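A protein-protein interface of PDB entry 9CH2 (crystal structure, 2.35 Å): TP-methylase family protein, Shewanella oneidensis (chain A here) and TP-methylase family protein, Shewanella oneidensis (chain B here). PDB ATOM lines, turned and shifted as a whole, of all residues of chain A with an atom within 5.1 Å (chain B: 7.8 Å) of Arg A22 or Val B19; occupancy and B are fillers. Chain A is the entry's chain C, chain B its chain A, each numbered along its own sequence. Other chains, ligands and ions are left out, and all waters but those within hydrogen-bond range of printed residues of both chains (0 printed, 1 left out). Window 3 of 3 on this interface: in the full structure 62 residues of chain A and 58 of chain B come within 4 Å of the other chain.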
ATOM      1  N   ALA A  14      14.557 -27.631 -20.675  1.00  0.00           N
ATOM      2  CA  ALA A  14      15.770 -27.900 -21.431  1.00  0.00           C
ATOM      3  C   ALA A  14      16.417 -26.613 -21.938  1.00  0.00           C
ATOM      4  O   ALA A  14      17.639 -26.491 -21.930  1.00  0.00           O
ATOM      5  CB  ALA A  14      15.455 -28.836 -22.578  1.00  0.00           C
ATOM      6  N   GLY A  15      15.591 -25.658 -22.379  1.00  0.00           N
ATOM      7  CA  GLY A  15      16.072 -24.545 -23.181  1.00  0.00           C
ATOM      8  C   GLY A  15      16.569 -23.366 -22.344  1.00  0.00           C
ATOM      9  O   GLY A  15      17.460 -22.638 -22.777  1.00  0.00           O
ATOM     10  N   ILE A  17      17.889 -23.218 -19.259  1.00  0.00           N
ATOM     11  CA  ILE A  17      19.041 -23.362 -18.384  1.00  0.00           C
ATOM     12  C   ILE A  17      20.243 -22.719 -19.070  1.00  0.00           C
ATOM     13  O   ILE A  17      20.358 -22.760 -20.293  1.00  0.00           O
ATOM     14  CB  ILE A  17      19.304 -24.838 -18.034  1.00  0.00           C
ATOM     15  CG1 ILE A  17      20.339 -24.971 -16.916  1.00  0.00           C
ATOM     16  CG2 ILE A  17      19.708 -25.634 -19.276  1.00  0.00           C
ATOM     17  CD1 ILE A  17      20.620 -26.403 -16.495  1.00  0.00           C
ATOM     18  N   SER A  18      21.131 -22.118 -18.268  1.00  0.00           N
ATOM     19  CA  SER A  18      22.330 -21.489 -18.795  1.00  0.00           C
ATOM     20  C   SER A  18      23.335 -22.565 -19.195  1.00  0.00           C
ATOM     21  O   SER A  18      23.282 -23.687 -18.698  1.00  0.00           O
ATOM     22  CB  SER A  18      22.930 -20.523 -17.802  1.00  0.00           C
ATOM     23  OG  SER A  18      23.531 -21.211 -16.714  1.00  0.00           O
ATOM     24  N   VAL A  19      24.253 -22.201 -20.098  1.00  0.00           N
ATOM     25  CA  VAL A  19      25.224 -23.140 -20.632  1.00  0.00           C
ATOM     26  C   VAL A  19      26.074 -23.690 -19.489  1.00  0.00           C
ATOM     27  O   VAL A  19      26.278 -24.898 -19.391  1.00  0.00           O
ATOM     28  CB  VAL A  19      26.102 -22.485 -21.715  1.00  0.00           C
ATOM     29  CG1 VAL A  19      27.228 -23.407 -22.165  1.00  0.00           C
ATOM     30  CG2 VAL A  19      25.275 -22.026 -22.910  1.00  0.00           C
ATOM     31  N   LEU A  20      26.567 -22.792 -18.630  1.00  0.00           N
ATOM     32  CA  LEU A  20      27.444 -23.180 -17.538  1.00  0.00           C
ATOM     33  C   LEU A  20      26.678 -24.067 -16.560  1.00  0.00           C
ATOM     34  O   LEU A  20      27.204 -25.069 -16.082  1.00  0.00           O
ATOM     35  CB  LEU A  20      28.006 -21.938 -16.846  1.00  0.00           C
ATOM     36  CG  LEU A  20      28.969 -22.197 -15.684  1.00  0.00           C
ATOM     37  CD1 LEU A  20      30.219 -22.922 -16.158  1.00  0.00           C
ATOM     38  CD2 LEU A  20      29.336 -20.900 -14.982  1.00  0.00           C
ATOM     39  N   SER A  21      25.429 -23.685 -16.273  1.00  0.00           N
ATOM     40  CA  SER A  21      24.621 -24.390 -15.291  1.00  0.00           C
ATOM     41  C   SER A  21      24.400 -25.834 -15.732  1.00  0.00           C
ATOM     42  O   SER A  21      24.416 -26.744 -14.907  1.00  0.00           O
ATOM     43  CB  SER A  21      23.315 -23.681 -15.046  1.00  0.00           C
ATOM     44  OG  SER A  21      23.529 -22.441 -14.387  1.00  0.00           O
ATOM     45  N   ARG A  22      24.195 -26.034 -17.037  1.00  0.00           N
ATOM     46  CA  ARG A  22      24.029 -27.373 -17.577  1.00  0.00           C
ATOM     47  C   ARG A  22      25.343 -28.135 -17.439  1.00  0.00           C
ATOM     48  O   ARG A  22      25.348 -29.321 -17.119  1.00  0.00           O
ATOM     49  CB  ARG A  22      23.575 -27.351 -19.041  1.00  0.00           C
ATOM     50  CG  ARG A  22      23.607 -28.726 -19.692  1.00  0.00           C
ATOM     51  CD  ARG A  22      22.648 -28.821 -20.866  1.00  0.00           C
ATOM     52  NE  ARG A  22      23.032 -27.922 -21.959  1.00  0.00           N
ATOM     53  CZ  ARG A  22      22.995 -28.242 -23.245  1.00  0.00           C
ATOM     54  NH1 ARG A  22      23.461 -27.400 -24.149  1.00  0.00           N
ATOM     55  NH2 ARG A  22      22.506 -29.410 -23.622  1.00  0.00           N
ATOM     56  N   SER A  23      26.454 -27.433 -17.688  1.00  0.00           N
ATOM     57  CA  SER A  23      27.777 -28.020 -17.568  1.00  0.00           C
ATOM     58  C   SER A  23      27.991 -28.516 -16.140  1.00  0.00           C
ATOM     59  O   SER A  23      28.581 -29.574 -15.930  1.00  0.00           O
ATOM     60  CB  SER A  23      28.846 -27.039 -17.981  1.00  0.00           C
ATOM     61  OG  SER A  23      30.134 -27.637 -17.958  1.00  0.00           O
ATOM     62  N   TYR A  24      27.493 -27.748 -15.164  1.00  0.00           N
ATOM     63  CA  TYR A  24      27.633 -28.105 -13.761  1.00  0.00           C
ATOM     64  C   TYR A  24      26.908 -29.421 -13.496  1.00  0.00           C
ATOM     65  O   TYR A  24      27.458 -30.319 -12.863  1.00  0.00           O
ATOM     66  CB  TYR A  24      27.125 -27.005 -12.823  1.00  0.00           C
ATOM     67  CG  TYR A  24      28.180 -25.983 -12.418  1.00  0.00           C
ATOM     68  CD1 TYR A  24      29.227 -26.339 -11.578  1.00  0.00           C
ATOM     69  CD2 TYR A  24      28.120 -24.665 -12.854  1.00  0.00           C
ATOM     70  CE1 TYR A  24      30.193 -25.422 -11.198  1.00  0.00           C
ATOM     71  CE2 TYR A  24      29.079 -23.737 -12.479  1.00  0.00           C
ATOM     72  CZ  TYR A  24      30.118 -24.116 -11.649  1.00  0.00           C
ATOM     73  OH  TYR A  24      31.067 -23.210 -11.274  1.00  0.00           O
ATOM     74  N   ILE A  25      25.664 -29.524 -13.979  1.00  0.00           N
ATOM     75  CA  ILE A  25      24.868 -30.723 -13.779  1.00  0.00           C
ATOM     76  C   ILE A  25      25.586 -31.905 -14.425  1.00  0.00           C
ATOM     77  O   ILE A  25      25.582 -33.011 -13.890  1.00  0.00           O
ATOM     78  CB  ILE A  25      23.448 -30.545 -14.347  1.00  0.00           C
ATOM     79  CG1 ILE A  25      22.665 -29.475 -13.589  1.00  0.00           C
ATOM     80  CG2 ILE A  25      22.700 -31.878 -14.370  1.00  0.00           C
ATOM     81  CD1 ILE A  25      21.273 -29.223 -14.139  1.00  0.00           C
ATOM     82  N   GLU A  26      26.215 -31.642 -15.573  1.00  0.00           N
ATOM     83  CA  GLU A  26      26.769 -32.690 -16.414  1.00  0.00           C
ATOM     84  C   GLU A  26      27.990 -33.320 -15.746  1.00  0.00           C
ATOM     85  O   GLU A  26      28.201 -34.525 -15.856  1.00  0.00           O
ATOM     86  CB  GLU A  26      27.111 -32.093 -17.780  1.00  0.00           C
ATOM     87  CG  GLU A  26      27.508 -33.133 -18.822  1.00  0.00           C
ATOM     88  CD  GLU A  26      27.726 -32.552 -20.208  1.00  0.00           C
ATOM     89  OE1 GLU A  26      26.769 -31.963 -20.754  1.00  0.00           O
ATOM     90  OE2 GLU A  26      28.848 -32.686 -20.739  1.00  0.00           O
ATOM     91  N   TRP A  43      14.711 -35.320 -18.502  1.00  0.00           N
ATOM     92  CA  TRP A  43      15.749 -34.518 -19.127  1.00  0.00           C
ATOM     93  C   TRP A  43      16.991 -34.491 -18.239  1.00  0.00           C
ATOM     94  O   TRP A  43      18.106 -34.688 -18.718  1.00  0.00           O
ATOM     95  CB  TRP A  43      15.227 -33.101 -19.404  1.00  0.00           C
ATOM     96  CG  TRP A  43      16.309 -32.066 -19.578  1.00  0.00           C
ATOM     97  CD1 TRP A  43      16.998 -31.774 -20.718  1.00  0.00           C
ATOM     98  CD2 TRP A  43      16.815 -31.173 -18.562  1.00  0.00           C
ATOM     99  NE1 TRP A  43      17.898 -30.769 -20.485  1.00  0.00           N
ATOM    100  CE2 TRP A  43      17.810 -30.379 -19.174  1.00  0.00           C
ATOM    101  CE3 TRP A  43      16.529 -30.968 -17.209  1.00  0.00           C
ATOM    102  CZ2 TRP A  43      18.514 -29.402 -18.475  1.00  0.00           C
ATOM    103  CZ3 TRP A  43      17.226 -30.001 -16.519  1.00  0.00           C
ATOM    104  CH2 TRP A  43      18.204 -29.230 -17.145  1.00  0.00           C
ATOM    105  N   LEU A  47      20.920 -36.365 -18.412  1.00  0.00           N
ATOM    106  CA  LEU A  47      22.050 -35.452 -18.418  1.00  0.00           C
ATOM    107  C   LEU A  47      23.065 -35.908 -17.373  1.00  0.00           C
ATOM    108  O   LEU A  47      24.271 -35.798 -17.578  1.00  0.00           O
ATOM    109  CB  LEU A  47      21.532 -34.041 -18.142  1.00  0.00           C
ATOM    110  CG  LEU A  47      22.207 -32.910 -18.924  1.00  0.00           C
ATOM    111  CD1 LEU A  47      21.613 -31.570 -18.521  1.00  0.00           C
ATOM    112  CD2 LEU A  47      23.713 -32.911 -18.737  1.00  0.00           C
ATOM    113  N   GLY B  15      29.007 -18.264 -20.670  1.00  0.00           N
ATOM    114  CA  GLY B  15      28.411 -19.332 -19.883  1.00  0.00           C
ATOM    115  C   GLY B  15      27.001 -19.010 -19.391  1.00  0.00           C
ATOM    116  O   GLY B  15      26.287 -19.905 -18.944  1.00  0.00           O
ATOM    117  N   GLN B  16      26.599 -17.738 -19.473  1.00  0.00           N
ATOM    118  CA  GLN B  16      25.406 -17.292 -18.770  1.00  0.00           C
ATOM    119  C   GLN B  16      24.246 -17.100 -19.746  1.00  0.00           C
ATOM    120  O   GLN B  16      23.160 -16.689 -19.345  1.00  0.00           O
ATOM    121  CB  GLN B  16      25.718 -16.026 -17.973  1.00  0.00           C
ATOM    122  CG  GLN B  16      24.814 -15.825 -16.761  1.00  0.00           C
ATOM    123  CD  GLN B  16      25.366 -14.828 -15.767  1.00  0.00           C
ATOM    124  OE1 GLN B  16      25.543 -13.643 -16.071  1.00  0.00           O
ATOM    125  NE2 GLN B  16      25.644 -15.302 -14.561  1.00  0.00           N
ATOM    126  N   ILE B  17      24.478 -17.418 -21.023  1.00  0.00           N
ATOM    127  CA  ILE B  17      23.414 -17.404 -22.015  1.00  0.00           C
ATOM    128  C   ILE B  17      22.647 -18.720 -21.918  1.00  0.00           C
ATOM    129  O   ILE B  17      23.221 -19.753 -21.578  1.00  0.00           O
ATOM    130  CB  ILE B  17      23.977 -17.176 -23.430  1.00  0.00           C
ATOM    131  CG1 ILE B  17      22.860 -17.018 -24.462  1.00  0.00           C
ATOM    132  CG2 ILE B  17      24.949 -18.291 -23.818  1.00  0.00           C
ATOM    133  CD1 ILE B  17      23.346 -16.654 -25.853  1.00  0.00           C
ATOM    134  N   SER B  18      21.345 -18.663 -22.217  1.00  0.00           N
ATOM    135  CA  SER B  18      20.498 -19.846 -22.211  1.00  0.00           C
ATOM    136  C   SER B  18      20.851 -20.734 -23.400  1.00  0.00           C
ATOM    137  O   SER B  18      21.316 -20.248 -24.428  1.00  0.00           O
ATOM    138  CB  SER B  18      19.039 -19.469 -22.227  1.00  0.00           C
ATOM    139  OG  SER B  18      18.704 -18.673 -21.098  1.00  0.00           O
ATOM    140  N   VAL B  19      20.618 -22.041 -23.245  1.00  0.00           N
ATOM    141  CA  VAL B  19      20.923 -23.005 -24.289  1.00  0.00           C
ATOM    142  C   VAL B  19      20.161 -22.633 -25.559  1.00  0.00           C
ATOM    143  O   VAL B  19      20.720 -22.670 -26.653  1.00  0.00           O
ATOM    144  CB  VAL B  19      20.596 -24.444 -23.846  1.00  0.00           C
ATOM    145  CG1 VAL B  19      20.722 -25.433 -24.998  1.00  0.00           C
ATOM    146  CG2 VAL B  19      21.455 -24.882 -22.666  1.00  0.00           C
ATOM    147  N   LEU B  20      18.883 -22.274 -25.401  1.00  0.00           N
ATOM    148  CA  LEU B  20      18.020 -21.996 -26.538  1.00  0.00           C
ATOM    149  C   LEU B  20      18.458 -20.701 -27.219  1.00  0.00           C
ATOM    150  O   LEU B  20      18.460 -20.612 -28.445  1.00  0.00           O
ATOM    151  CB  LEU B  20      16.561 -21.925 -26.088  1.00  0.00           C
ATOM    152  CG  LEU B  20      15.533 -21.674 -27.196  1.00  0.00           C
ATOM    153  CD1 LEU B  20      15.576 -22.780 -28.236  1.00  0.00           C
ATOM    154  CD2 LEU B  20      14.130 -21.530 -26.628  1.00  0.00           C
ATOM    155  N   SER B  21      18.826 -19.699 -26.415  1.00  0.00           N
ATOM    156  CA  SER B  21      19.195 -18.396 -26.945  1.00  0.00           C
ATOM    157  C   SER B  21      20.460 -18.515 -27.791  1.00  0.00           C
ATOM    158  O   SER B  21      20.578 -17.878 -28.835  1.00  0.00           O
ATOM    159  CB  SER B  21      19.364 -17.380 -25.843  1.00  0.00           C
ATOM    160  OG  SER B  21      18.114 -17.060 -25.246  1.00  0.00           O
ATOM    161  N   ARG B  22      21.399 -19.344 -27.326  1.00  0.00           N
ATOM    162  CA  ARG B  22      22.651 -19.569 -28.029  1.00  0.00           C
ATOM    163  C   ARG B  22      22.365 -20.264 -29.357  1.00  0.00           C
ATOM    164  O   ARG B  22      23.049 -20.022 -30.349  1.00  0.00           O
ATOM    165  CB  ARG B  22      23.585 -20.373 -27.119  1.00  0.00           C
ATOM    166  CG  ARG B  22      24.900 -20.830 -27.735  1.00  0.00           C
ATOM    167  CD  ARG B  22      25.866 -21.215 -26.626  1.00  0.00           C
ATOM    168  NE  ARG B  22      26.883 -22.191 -27.029  1.00  0.00           N
ATOM    169  CZ  ARG B  22      26.956 -23.421 -26.537  1.00  0.00           C
ATOM    170  NH1 ARG B  22      27.957 -24.215 -26.874  1.00  0.00           N
ATOM    171  NH2 ARG B  22      26.036 -23.848 -25.690  1.00  0.00           N
ATOM    172  N   SER B  23      21.337 -21.119 -29.359  1.00  0.00           N
ATOM    173  CA  SER B  23      20.906 -21.815 -30.560  1.00  0.00           C
ATOM    174  C   SER B  23      20.367 -20.815 -31.582  1.00  0.00           C
ATOM    175  O   SER B  23      20.602 -20.961 -32.779  1.00  0.00           O
ATOM    176  CB  SER B  23      19.879 -22.871 -30.232  1.00  0.00           C
ATOM    177  OG  SER B  23      19.511 -23.609 -31.390  1.00  0.00           O
ATOM    178  N   TYR B  24      19.645 -19.799 -31.096  1.00  0.00           N
ATOM    179  CA  TYR B  24      19.069 -18.787 -31.968  1.00  0.00           C
ATOM    180  C   TYR B  24      20.182 -18.034 -32.691  1.00  0.00           C
ATOM    181  O   TYR B  24      20.076 -17.770 -33.887  1.00  0.00           O
ATOM    182  CB  TYR B  24      18.166 -17.819 -31.197  1.00  0.00           C
ATOM    183  CG  TYR B  24      16.705 -18.247 -31.148  1.00  0.00           C
ATOM    184  CD1 TYR B  24      15.884 -18.102 -32.259  1.00  0.00           C
ATOM    185  CD2 TYR B  24      16.148 -18.791 -29.997  1.00  0.00           C
ATOM    186  CE1 TYR B  24      14.556 -18.490 -32.232  1.00  0.00           C
ATOM    187  CE2 TYR B  24      14.819 -19.182 -29.956  1.00  0.00           C
ATOM    188  CZ  TYR B  24      14.021 -19.031 -31.076  1.00  0.00           C
ATOM    189  OH  TYR B  24      12.712 -19.413 -31.047  1.00  0.00           O
ATOM    190  N   ILE B  25      21.240 -17.683 -31.955  1.00  0.00           N
ATOM    191  CA  ILE B  25      22.359 -16.953 -32.527  1.00  0.00           C
ATOM    192  C   ILE B  25      23.010 -17.811 -33.607  1.00  0.00           C
ATOM    193  O   ILE B  25      23.387 -17.311 -34.665  1.00  0.00           O
ATOM    194  CB  ILE B  25      23.375 -16.556 -31.440  1.00  0.00           C
ATOM    195  CG1 ILE B  25      22.763 -15.601 -30.415  1.00  0.00           C
ATOM    196  CG2 ILE B  25      24.642 -15.976 -32.068  1.00  0.00           C
ATOM    197  CD1 ILE B  25      23.700 -15.229 -29.280  1.00  0.00           C
ATOM    198  N   GLU B  26      23.125 -19.110 -33.323  1.00  0.00           N
ATOM    199  CA  GLU B  26      23.912 -20.018 -34.140  1.00  0.00           C
ATOM    200  C   GLU B  26      23.208 -20.262 -35.473  1.00  0.00           C
ATOM    201  O   GLU B  26      23.861 -20.389 -36.505  1.00  0.00           O
ATOM    202  CB  GLU B  26      24.136 -21.305 -33.345  1.00  0.00           C
ATOM    203  CG  GLU B  26      25.392 -22.069 -33.755  1.00  0.00           C
ATOM    204  CD  GLU B  26      25.745 -23.207 -32.813  1.00  0.00           C
ATOM    205  OE1 GLU B  26      25.000 -23.411 -31.831  1.00  0.00           O
ATOM    206  OE2 GLU B  26      26.764 -23.887 -33.059  1.00  0.00           O
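The backbone carbonyl oxygen (O) of Gly B15 lies within hydrogen-bond range of the backbone NH (N) of Val A19 (3.3 Å). The backbone NH (N) of Leu A20 lies within hydrogen-bond range of the backbone carbonyl oxygen (O) of Gly B15. The backbone NH (N) of Val A19 sits at hydrogen-bond distance from the backbone carbonyl oxygen (O) of Ile B17, at 3.0 Å. N of Val B19 sits at hydrogen-bond distance from O of Gly A15, 3.2 Å away. The backbone NH (N) of Val B19 lies within hydrogen-bond range of the backbone carbonyl oxygen (O) of Ile A17 (3.0 Å). The backbone carbonyl oxygen of Gly A15 sits at hydrogen-bond distance from the backbone NH of Leu B20 (3.0 Å).
The side-chain hydroxyl (OG) of Ser A18 sits at hydrogen-bond distance from the side-chain hydroxyl (OG) of Ser A21 (2.6 Å).
Among the printed residues, merely in contact across the chains: Gly A15 with Ser B18 (3.6 Å), Ile A17 with Ser B18 (3.5 Å), Ser A18 with Gly B15 (3.6 Å), Ser A18 with Ile B17 (3.4 Å), Val A19 with Arg B22 (3.4 Å) and Arg A22 with Val B19 (3.5 Å).
Arg A22 touches one residue of chain B. Of chain A, only Gly A15, Ile A17 and Arg A22 come within 4 Å of Val B19. Printed residues of chain B within 4 Å of Val A19: Gly B15 (3.3 Å), Ile B17 (3.0 Å) and Arg B22 (3.4 Å). Printed residues of chain A within 4 Å of Leu B20: Gly A15 (3.0 Å). Tyr A24 touches none of the printed residues of chain B. The nearest residue of chain A that does not touch Val B19 is Ala A14 (4.1 Å). The nearest printed residue of chain B that does not touch Val A19 is Ser B18 (4.6 Å).
Of the 14 printed residues of chain A, 6 touch a printed residue of chain B. Hydrophobic or aromatic side chains of chain A within 4 Å of the printed part of chain B: Ile A17, Val A19 and Leu A20. Of the 12 printed residues of chain B, 6 touch a printed residue of chain A.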
